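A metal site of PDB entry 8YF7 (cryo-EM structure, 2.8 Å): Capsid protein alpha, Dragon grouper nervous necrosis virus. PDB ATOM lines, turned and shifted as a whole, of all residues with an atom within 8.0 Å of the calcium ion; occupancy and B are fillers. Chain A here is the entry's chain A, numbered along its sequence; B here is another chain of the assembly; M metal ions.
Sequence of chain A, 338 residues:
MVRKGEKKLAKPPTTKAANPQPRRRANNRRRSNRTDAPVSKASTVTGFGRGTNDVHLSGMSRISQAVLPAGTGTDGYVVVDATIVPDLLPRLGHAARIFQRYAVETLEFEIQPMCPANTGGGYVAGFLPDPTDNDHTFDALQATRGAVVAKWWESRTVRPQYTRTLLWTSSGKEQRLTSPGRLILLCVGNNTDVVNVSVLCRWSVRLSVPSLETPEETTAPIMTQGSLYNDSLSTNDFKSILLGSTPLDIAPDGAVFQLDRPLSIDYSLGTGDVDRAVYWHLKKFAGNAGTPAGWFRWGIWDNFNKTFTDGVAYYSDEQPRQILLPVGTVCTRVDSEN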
ATOM      1  N   ALA A  96     -30.543 -27.433 -31.293  1.00  0.00           N
ATOM      2  CA  ALA A  96     -29.988 -27.043 -30.005  1.00  0.00           C
ATOM      3  C   ALA A  96     -30.733 -25.855 -29.420  1.00  0.00           C
ATOM      4  O   ALA A  96     -30.693 -25.626 -28.211  1.00  0.00           O
ATOM      5  CB  ALA A  96     -28.507 -26.716 -30.147  1.00  0.00           C
ATOM      6  N   ARG A  97     -31.496 -25.142 -30.238  1.00  0.00           N
ATOM      7  CA  ARG A  97     -32.289 -24.064 -29.673  1.00  0.00           C
ATOM      8  C   ARG A  97     -33.478 -24.659 -28.939  1.00  0.00           C
ATOM      9  O   ARG A  97     -34.011 -24.037 -28.032  1.00  0.00           O
ATOM     10  CB  ARG A  97     -32.743 -23.081 -30.742  1.00  0.00           C
ATOM     11  CG  ARG A  97     -33.336 -21.818 -30.174  1.00  0.00           C
ATOM     12  CD  ARG A  97     -33.350 -20.696 -31.191  1.00  0.00           C
ATOM     13  NE  ARG A  97     -33.913 -19.472 -30.614  1.00  0.00           N
ATOM     14  CZ  ARG A  97     -34.018 -18.320 -31.273  1.00  0.00           C
ATOM     15  NH1 ARG A  97     -33.599 -18.234 -32.522  1.00  0.00           N
ATOM     16  NH2 ARG A  97     -34.537 -17.264 -30.672  1.00  0.00           N
ATOM     17  N   PHE A  99     -33.242 -27.589 -27.219  1.00  0.00           N
ATOM     18  CA  PHE A  99     -32.735 -28.590 -26.292  1.00  0.00           C
ATOM     19  C   PHE A  99     -31.673 -27.988 -25.389  1.00  0.00           C
ATOM     20  O   PHE A  99     -31.127 -26.920 -25.672  1.00  0.00           O
ATOM     21  CB  PHE A  99     -32.148 -29.803 -27.038  1.00  0.00           C
ATOM     22  CG  PHE A  99     -33.177 -30.840 -27.397  1.00  0.00           C
ATOM     23  CD1 PHE A  99     -33.690 -31.685 -26.442  1.00  0.00           C
ATOM     24  CD2 PHE A  99     -33.614 -30.970 -28.704  1.00  0.00           C
ATOM     25  CE1 PHE A  99     -34.628 -32.634 -26.771  1.00  0.00           C
ATOM     26  CE2 PHE A  99     -34.551 -31.919 -29.033  1.00  0.00           C
ATOM     27  CZ  PHE A  99     -35.052 -32.748 -28.065  1.00  0.00           C
ATOM     28  N   GLN A 100     -31.382 -28.681 -24.284  1.00  0.00           N
ATOM     29  CA  GLN A 100     -30.349 -28.238 -23.354  1.00  0.00           C
ATOM     30  C   GLN A 100     -29.018 -28.957 -23.541  1.00  0.00           C
ATOM     31  O   GLN A 100     -27.976 -28.302 -23.529  1.00  0.00           O
ATOM     32  CB  GLN A 100     -30.794 -28.428 -21.904  1.00  0.00           C
ATOM     33  CG  GLN A 100     -31.913 -27.518 -21.455  1.00  0.00           C
ATOM     34  CD  GLN A 100     -31.439 -26.162 -21.000  1.00  0.00           C
ATOM     35  OE1 GLN A 100     -30.303 -25.769 -21.269  1.00  0.00           O
ATOM     36  NE2 GLN A 100     -32.291 -25.437 -20.287  1.00  0.00           N
ATOM     37  N   ARG A 101     -29.033 -30.282 -23.709  1.00  0.00           N
ATOM     38  CA  ARG A 101     -27.787 -31.033 -23.802  1.00  0.00           C
ATOM     39  C   ARG A 101     -27.704 -31.745 -25.145  1.00  0.00           C
ATOM     40  O   ARG A 101     -28.718 -32.124 -25.732  1.00  0.00           O
ATOM     41  CB  ARG A 101     -27.671 -32.064 -22.670  1.00  0.00           C
ATOM     42  CG  ARG A 101     -27.987 -31.509 -21.297  1.00  0.00           C
ATOM     43  CD  ARG A 101     -26.908 -30.572 -20.821  1.00  0.00           C
ATOM     44  NE  ARG A 101     -25.628 -31.242 -20.619  1.00  0.00           N
ATOM     45  CZ  ARG A 101     -25.358 -32.059 -19.609  1.00  0.00           C
ATOM     46  NH1 ARG A 101     -26.260 -32.334 -18.689  1.00  0.00           N
ATOM     47  NH2 ARG A 101     -24.154 -32.610 -19.531  1.00  0.00           N
ATOM     48  N   TRP A 168     -23.272 -29.040 -23.618  1.00  0.00           N
ATOM     49  CA  TRP A 168     -24.343 -28.082 -23.395  1.00  0.00           C
ATOM     50  C   TRP A 168     -24.583 -27.271 -24.666  1.00  0.00           C
ATOM     51  O   TRP A 168     -23.631 -26.744 -25.250  1.00  0.00           O
ATOM     52  CB  TRP A 168     -23.998 -27.144 -22.242  1.00  0.00           C
ATOM     53  CG  TRP A 168     -23.906 -27.814 -20.908  1.00  0.00           C
ATOM     54  CD1 TRP A 168     -22.842 -28.510 -20.428  1.00  0.00           C
ATOM     55  CD2 TRP A 168     -24.904 -27.840 -19.883  1.00  0.00           C
ATOM     56  NE1 TRP A 168     -23.114 -28.977 -19.166  1.00  0.00           N
ATOM     57  CE2 TRP A 168     -24.380 -28.572 -18.813  1.00  0.00           C
ATOM     58  CE3 TRP A 168     -26.192 -27.306 -19.775  1.00  0.00           C
ATOM     59  CZ2 TRP A 168     -25.097 -28.803 -17.644  1.00  0.00           C
ATOM     60  CZ3 TRP A 168     -26.904 -27.527 -18.615  1.00  0.00           C
ATOM     61  CH2 TRP A 168     -26.357 -28.265 -17.560  1.00  0.00           C
ATOM     62  N   THR A 169     -25.845 -27.189 -25.076  1.00  0.00           N
ATOM     63  CA  THR A 169     -26.176 -26.480 -26.305  1.00  0.00           C
ATOM     64  C   THR A 169     -25.920 -24.979 -26.184  1.00  0.00           C
ATOM     65  O   THR A 169     -25.418 -24.359 -27.127  1.00  0.00           O
ATOM     66  CB  THR A 169     -27.624 -26.742 -26.691  1.00  0.00           C
ATOM     67  OG1 THR A 169     -28.484 -26.256 -25.655  1.00  0.00           O
ATOM     68  CG2 THR A 169     -27.861 -28.225 -26.869  1.00  0.00           C
ATOM     69  N   SER A 170     -26.256 -24.399 -25.044  1.00  0.00           N
ATOM     70  CA  SER A 170     -26.077 -22.974 -24.828  1.00  0.00           C
ATOM     71  C   SER A 170     -24.670 -22.675 -24.319  1.00  0.00           C
ATOM     72  O   SER A 170     -24.028 -23.505 -23.660  1.00  0.00           O
ATOM     73  CB  SER A 170     -27.112 -22.440 -23.845  1.00  0.00           C
ATOM     74  OG  SER A 170     -26.924 -22.989 -22.552  1.00  0.00           O
ATOM     75  N   SER A 171     -24.187 -21.476 -24.630  1.00  0.00           N
ATOM     76  CA  SER A 171     -22.842 -21.071 -24.273  1.00  0.00           C
ATOM     77  C   SER A 171     -22.732 -20.800 -22.781  1.00  0.00           C
ATOM     78  O   SER A 171     -23.718 -20.599 -22.067  1.00  0.00           O
ATOM     79  CB  SER A 171     -22.431 -19.832 -25.066  1.00  0.00           C
ATOM     80  OG  SER A 171     -21.125 -19.417 -24.708  1.00  0.00           O
ATOM     81  N   VAL A 209     -32.774 -33.238 -22.582  1.00  0.00           N
ATOM     82  CA  VAL A 209     -33.249 -32.176 -21.682  1.00  0.00           C
ATOM     83  C   VAL A 209     -33.954 -31.086 -22.485  1.00  0.00           C
ATOM     84  O   VAL A 209     -33.351 -30.043 -22.764  1.00  0.00           O
ATOM     85  CB  VAL A 209     -32.110 -31.613 -20.832  1.00  0.00           C
ATOM     86  CG1 VAL A 209     -32.652 -30.706 -19.749  1.00  0.00           C
ATOM     87  CG2 VAL A 209     -31.307 -32.743 -20.211  1.00  0.00           C
ATOM     88  N   SER A 211     -35.903 -27.892 -23.843  1.00  0.00           N
ATOM     89  CA  SER A 211     -36.083 -26.516 -23.394  1.00  0.00           C
ATOM     90  C   SER A 211     -36.357 -25.668 -24.611  1.00  0.00           C
ATOM     91  O   SER A 211     -36.585 -26.173 -25.715  1.00  0.00           O
ATOM     92  CB  SER A 211     -34.863 -26.013 -22.636  1.00  0.00           C
ATOM     93  OG  SER A 211     -33.739 -25.913 -23.488  1.00  0.00           O
ATOM     94  N   LEU A 212     -36.348 -24.343 -24.423  1.00  0.00           N
ATOM     95  CA  LEU A 212     -36.485 -23.381 -25.508  1.00  0.00           C
ATOM     96  C   LEU A 212     -35.536 -22.215 -25.243  1.00  0.00           C
ATOM     97  O   LEU A 212     -35.852 -21.260 -24.538  1.00  0.00           O
ATOM     98  CB  LEU A 212     -37.936 -22.906 -25.664  1.00  0.00           C
ATOM     99  CG  LEU A 212     -38.160 -22.030 -26.881  1.00  0.00           C
ATOM    100  CD1 LEU A 212     -37.737 -22.753 -28.141  1.00  0.00           C
ATOM    101  CD2 LEU A 212     -39.611 -21.620 -26.984  1.00  0.00           C
ATOM    102  N   GLU A 213     -34.340 -22.302 -25.815  1.00  0.00           N
ATOM    103  CA  GLU A 213     -33.300 -21.315 -25.555  1.00  0.00           C
ATOM    104  C   GLU A 213     -33.374 -20.157 -26.547  1.00  0.00           C
ATOM    105  O   GLU A 213     -34.094 -20.193 -27.554  1.00  0.00           O
ATOM    106  CB  GLU A 213     -31.931 -21.977 -25.620  1.00  0.00           C
ATOM    107  CG  GLU A 213     -31.794 -23.189 -24.726  1.00  0.00           C
ATOM    108  CD  GLU A 213     -30.494 -23.930 -24.939  1.00  0.00           C
ATOM    109  OE1 GLU A 213     -29.909 -23.801 -26.035  1.00  0.00           O
ATOM    110  OE2 GLU A 213     -30.057 -24.643 -24.014  1.00  0.00           O
ATOM    111  N   THR A 214     -32.628 -19.105 -26.235  1.00  0.00           N
ATOM    112  CA  THR A 214     -32.510 -17.911 -27.058  1.00  0.00           C
ATOM    113  C   THR A 214     -31.048 -17.655 -27.378  1.00  0.00           C
ATOM    114  O   THR A 214     -30.160 -18.017 -26.589  1.00  0.00           O
ATOM    115  CB  THR A 214     -33.106 -16.685 -26.345  1.00  0.00           C
ATOM    116  OG1 THR A 214     -32.401 -16.436 -25.130  1.00  0.00           O
ATOM    117  CG2 THR A 214     -34.575 -16.908 -26.047  1.00  0.00           C
ATOM    118  N   LEU B 128     -35.591 -24.531 -14.757  1.00  0.00           N
ATOM    119  CA  LEU B 128     -34.637 -24.677 -15.840  1.00  0.00           C
ATOM    120  C   LEU B 128     -33.448 -25.490 -15.348  1.00  0.00           C
ATOM    121  O   LEU B 128     -32.791 -25.094 -14.374  1.00  0.00           O
ATOM    122  CB  LEU B 128     -34.160 -23.313 -16.332  1.00  0.00           C
ATOM    123  CG  LEU B 128     -35.195 -22.230 -16.587  1.00  0.00           C
ATOM    124  CD1 LEU B 128     -34.515 -20.952 -17.048  1.00  0.00           C
ATOM    125  CD2 LEU B 128     -36.209 -22.685 -17.604  1.00  0.00           C
ATOM    126  N   PRO B 129     -33.132 -26.624 -15.987  1.00  0.00           N
ATOM    127  CA  PRO B 129     -31.983 -27.434 -15.545  1.00  0.00           C
ATOM    128  C   PRO B 129     -30.640 -26.804 -15.873  1.00  0.00           C
ATOM    129  O   PRO B 129     -29.608 -27.403 -15.537  1.00  0.00           O
ATOM    130  CB  PRO B 129     -32.167 -28.751 -16.311  1.00  0.00           C
ATOM    131  CG  PRO B 129     -33.591 -28.748 -16.759  1.00  0.00           C
ATOM    132  CD  PRO B 129     -33.923 -27.314 -17.006  1.00  0.00           C
ATOM    133  N   ASP B 130     -30.620 -25.654 -16.522  1.00  0.00           N
ATOM    134  CA  ASP B 130     -29.381 -24.965 -16.834  1.00  0.00           C
ATOM    135  C   ASP B 130     -29.242 -23.756 -15.923  1.00  0.00           C
ATOM    136  O   ASP B 130     -30.009 -22.791 -16.059  1.00  0.00           O
ATOM    137  CB  ASP B 130     -29.367 -24.525 -18.292  1.00  0.00           C
ATOM    138  CG  ASP B 130     -27.974 -24.232 -18.805  1.00  0.00           C
ATOM    139  OD1 ASP B 130     -27.078 -23.987 -17.976  1.00  0.00           O
ATOM    140  OD2 ASP B 130     -27.786 -24.231 -20.036  1.00  0.00           O
ATOM    141  N   PRO B 131     -28.306 -23.764 -14.975  1.00  0.00           N
ATOM    142  CA  PRO B 131     -28.125 -22.574 -14.125  1.00  0.00           C
ATOM    143  C   PRO B 131     -27.731 -21.342 -14.902  1.00  0.00           C
ATOM    144  O   PRO B 131     -28.077 -20.221 -14.497  1.00  0.00           O
ATOM    145  CB  PRO B 131     -27.029 -23.010 -13.140  1.00  0.00           C
ATOM    146  CG  PRO B 131     -26.380 -24.202 -13.768  1.00  0.00           C
ATOM    147  CD  PRO B 131     -27.425 -24.885 -14.572  1.00  0.00           C
ATOM    148  N   THR B 132     -27.027 -21.503 -16.024  1.00  0.00           N
ATOM    149  CA  THR B 132     -26.523 -20.343 -16.762  1.00  0.00           C
ATOM    150  C   THR B 132     -27.614 -19.647 -17.567  1.00  0.00           C
ATOM    151  O   THR B 132     -27.578 -18.418 -17.721  1.00  0.00           O
ATOM    152  CB  THR B 132     -25.377 -20.764 -17.679  1.00  0.00           C
ATOM    153  OG1 THR B 132     -25.844 -21.751 -18.614  1.00  0.00           O
ATOM    154  CG2 THR B 132     -24.230 -21.330 -16.874  1.00  0.00           C
ATOM    155  N   ASP B 133     -28.585 -20.392 -18.094  1.00  0.00           N
ATOM    156  CA  ASP B 133     -29.607 -19.786 -18.932  1.00  0.00           C
ATOM    157  C   ASP B 133     -30.432 -18.781 -18.146  1.00  0.00           C
ATOM    158  O   ASP B 133     -30.985 -19.093 -17.080  1.00  0.00           O
ATOM    159  CB  ASP B 133     -30.530 -20.851 -19.533  1.00  0.00           C
ATOM    160  CG  ASP B 133     -29.834 -21.707 -20.580  1.00  0.00           C
ATOM    161  OD1 ASP B 133     -28.894 -21.205 -21.228  1.00  0.00           O
ATOM    162  OD2 ASP B 133     -30.248 -22.874 -20.767  1.00  0.00           O
ATOM    163  N   ASN B 134     -30.537 -17.561 -18.684  1.00  0.00           N
ATOM    164  CA  ASN B 134     -31.301 -16.471 -18.091  1.00  0.00           C
ATOM    165  C   ASN B 134     -32.476 -16.071 -18.971  1.00  0.00           C
ATOM    166  O   ASN B 134     -32.793 -14.884 -19.085  1.00  0.00           O
ATOM    167  CB  ASN B 134     -30.401 -15.272 -17.807  1.00  0.00           C
ATOM    168  CG  ASN B 134     -29.255 -15.605 -16.864  1.00  0.00           C
ATOM    169  OD1 ASN B 134     -29.468 -16.184 -15.791  1.00  0.00           O
ATOM    170  ND2 ASN B 134     -28.045 -15.248 -17.258  1.00  0.00           N
ATOM    171  N   ARG B 176     -22.357 -24.344 -13.891  1.00  0.00           N
ATOM    172  CA  ARG B 176     -22.982 -25.589 -14.303  1.00  0.00           C
ATOM    173  C   ARG B 176     -22.461 -26.795 -13.531  1.00  0.00           C
ATOM    174  O   ARG B 176     -23.085 -27.860 -13.576  1.00  0.00           O
ATOM    175  CB  ARG B 176     -22.775 -25.800 -15.802  1.00  0.00           C
ATOM    176  CG  ARG B 176     -23.540 -24.796 -16.627  1.00  0.00           C
ATOM    177  CD  ARG B 176     -23.323 -24.989 -18.104  1.00  0.00           C
ATOM    178  NE  ARG B 176     -24.074 -23.982 -18.854  1.00  0.00           N
ATOM    179  CZ  ARG B 176     -24.029 -23.846 -20.174  1.00  0.00           C
ATOM    180  NH1 ARG B 176     -23.180 -24.528 -20.910  1.00  0.00           N
ATOM    181  NH2 ARG B 176     -24.852 -22.982 -20.753  1.00  0.00           N
HETATM  182 CA    CA M   1     -28.890 -24.081 -22.077  1.00  0.00          CA
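OD1 of Asp 130 of chain B sits at hydrogen-bond distance from OG1 of Thr 132 of chain B (2.6 Å).
The side-chain hydroxyl (OG1) of Thr 169 is in hydrogen-bond range of the side-chain carboxylate (OE1) of Glu 213 (2.9 Å).
OD1 of Asp 130 of chain B is in salt-bridge range of NE of Arg 176 of chain B (3.1 Å).
N of Gln 100 lies within hydrogen-bond range of O of Val 209, 2.8 Å away.
N of Glu 213 sits at hydrogen-bond distance from O of Arg 97, at 2.8 Å.
N of Thr 169 lies within hydrogen-bond range of O of Gln 100 (2.9 Å).
O of Ser 170 sits at hydrogen-bond distance from NH1 of Arg 176 of chain B.
Of the 22 residues printed, 5 come within 4 Å of the calcium ion.
OD2 of Asp 133 of chain B binds the calcium ion (2.2 Å).
OG of Ser 170 binds the calcium ion (2.3 Å).
OD2 of Asp 130 of chain B binds the calcium ion, at 2.3 Å.
The calcium ion is bound by OE2 of Glu 213, at 2.3 Å.
The calcium ion is bound by OE1 of Gln 100, 2.3 Å away.
The calcium ion has five donor atoms within binding distance.
Slightly farther from the calcium ion lies the side-chain carboxylate (OD1) of Asp 133 of chain B (3.0 Å).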
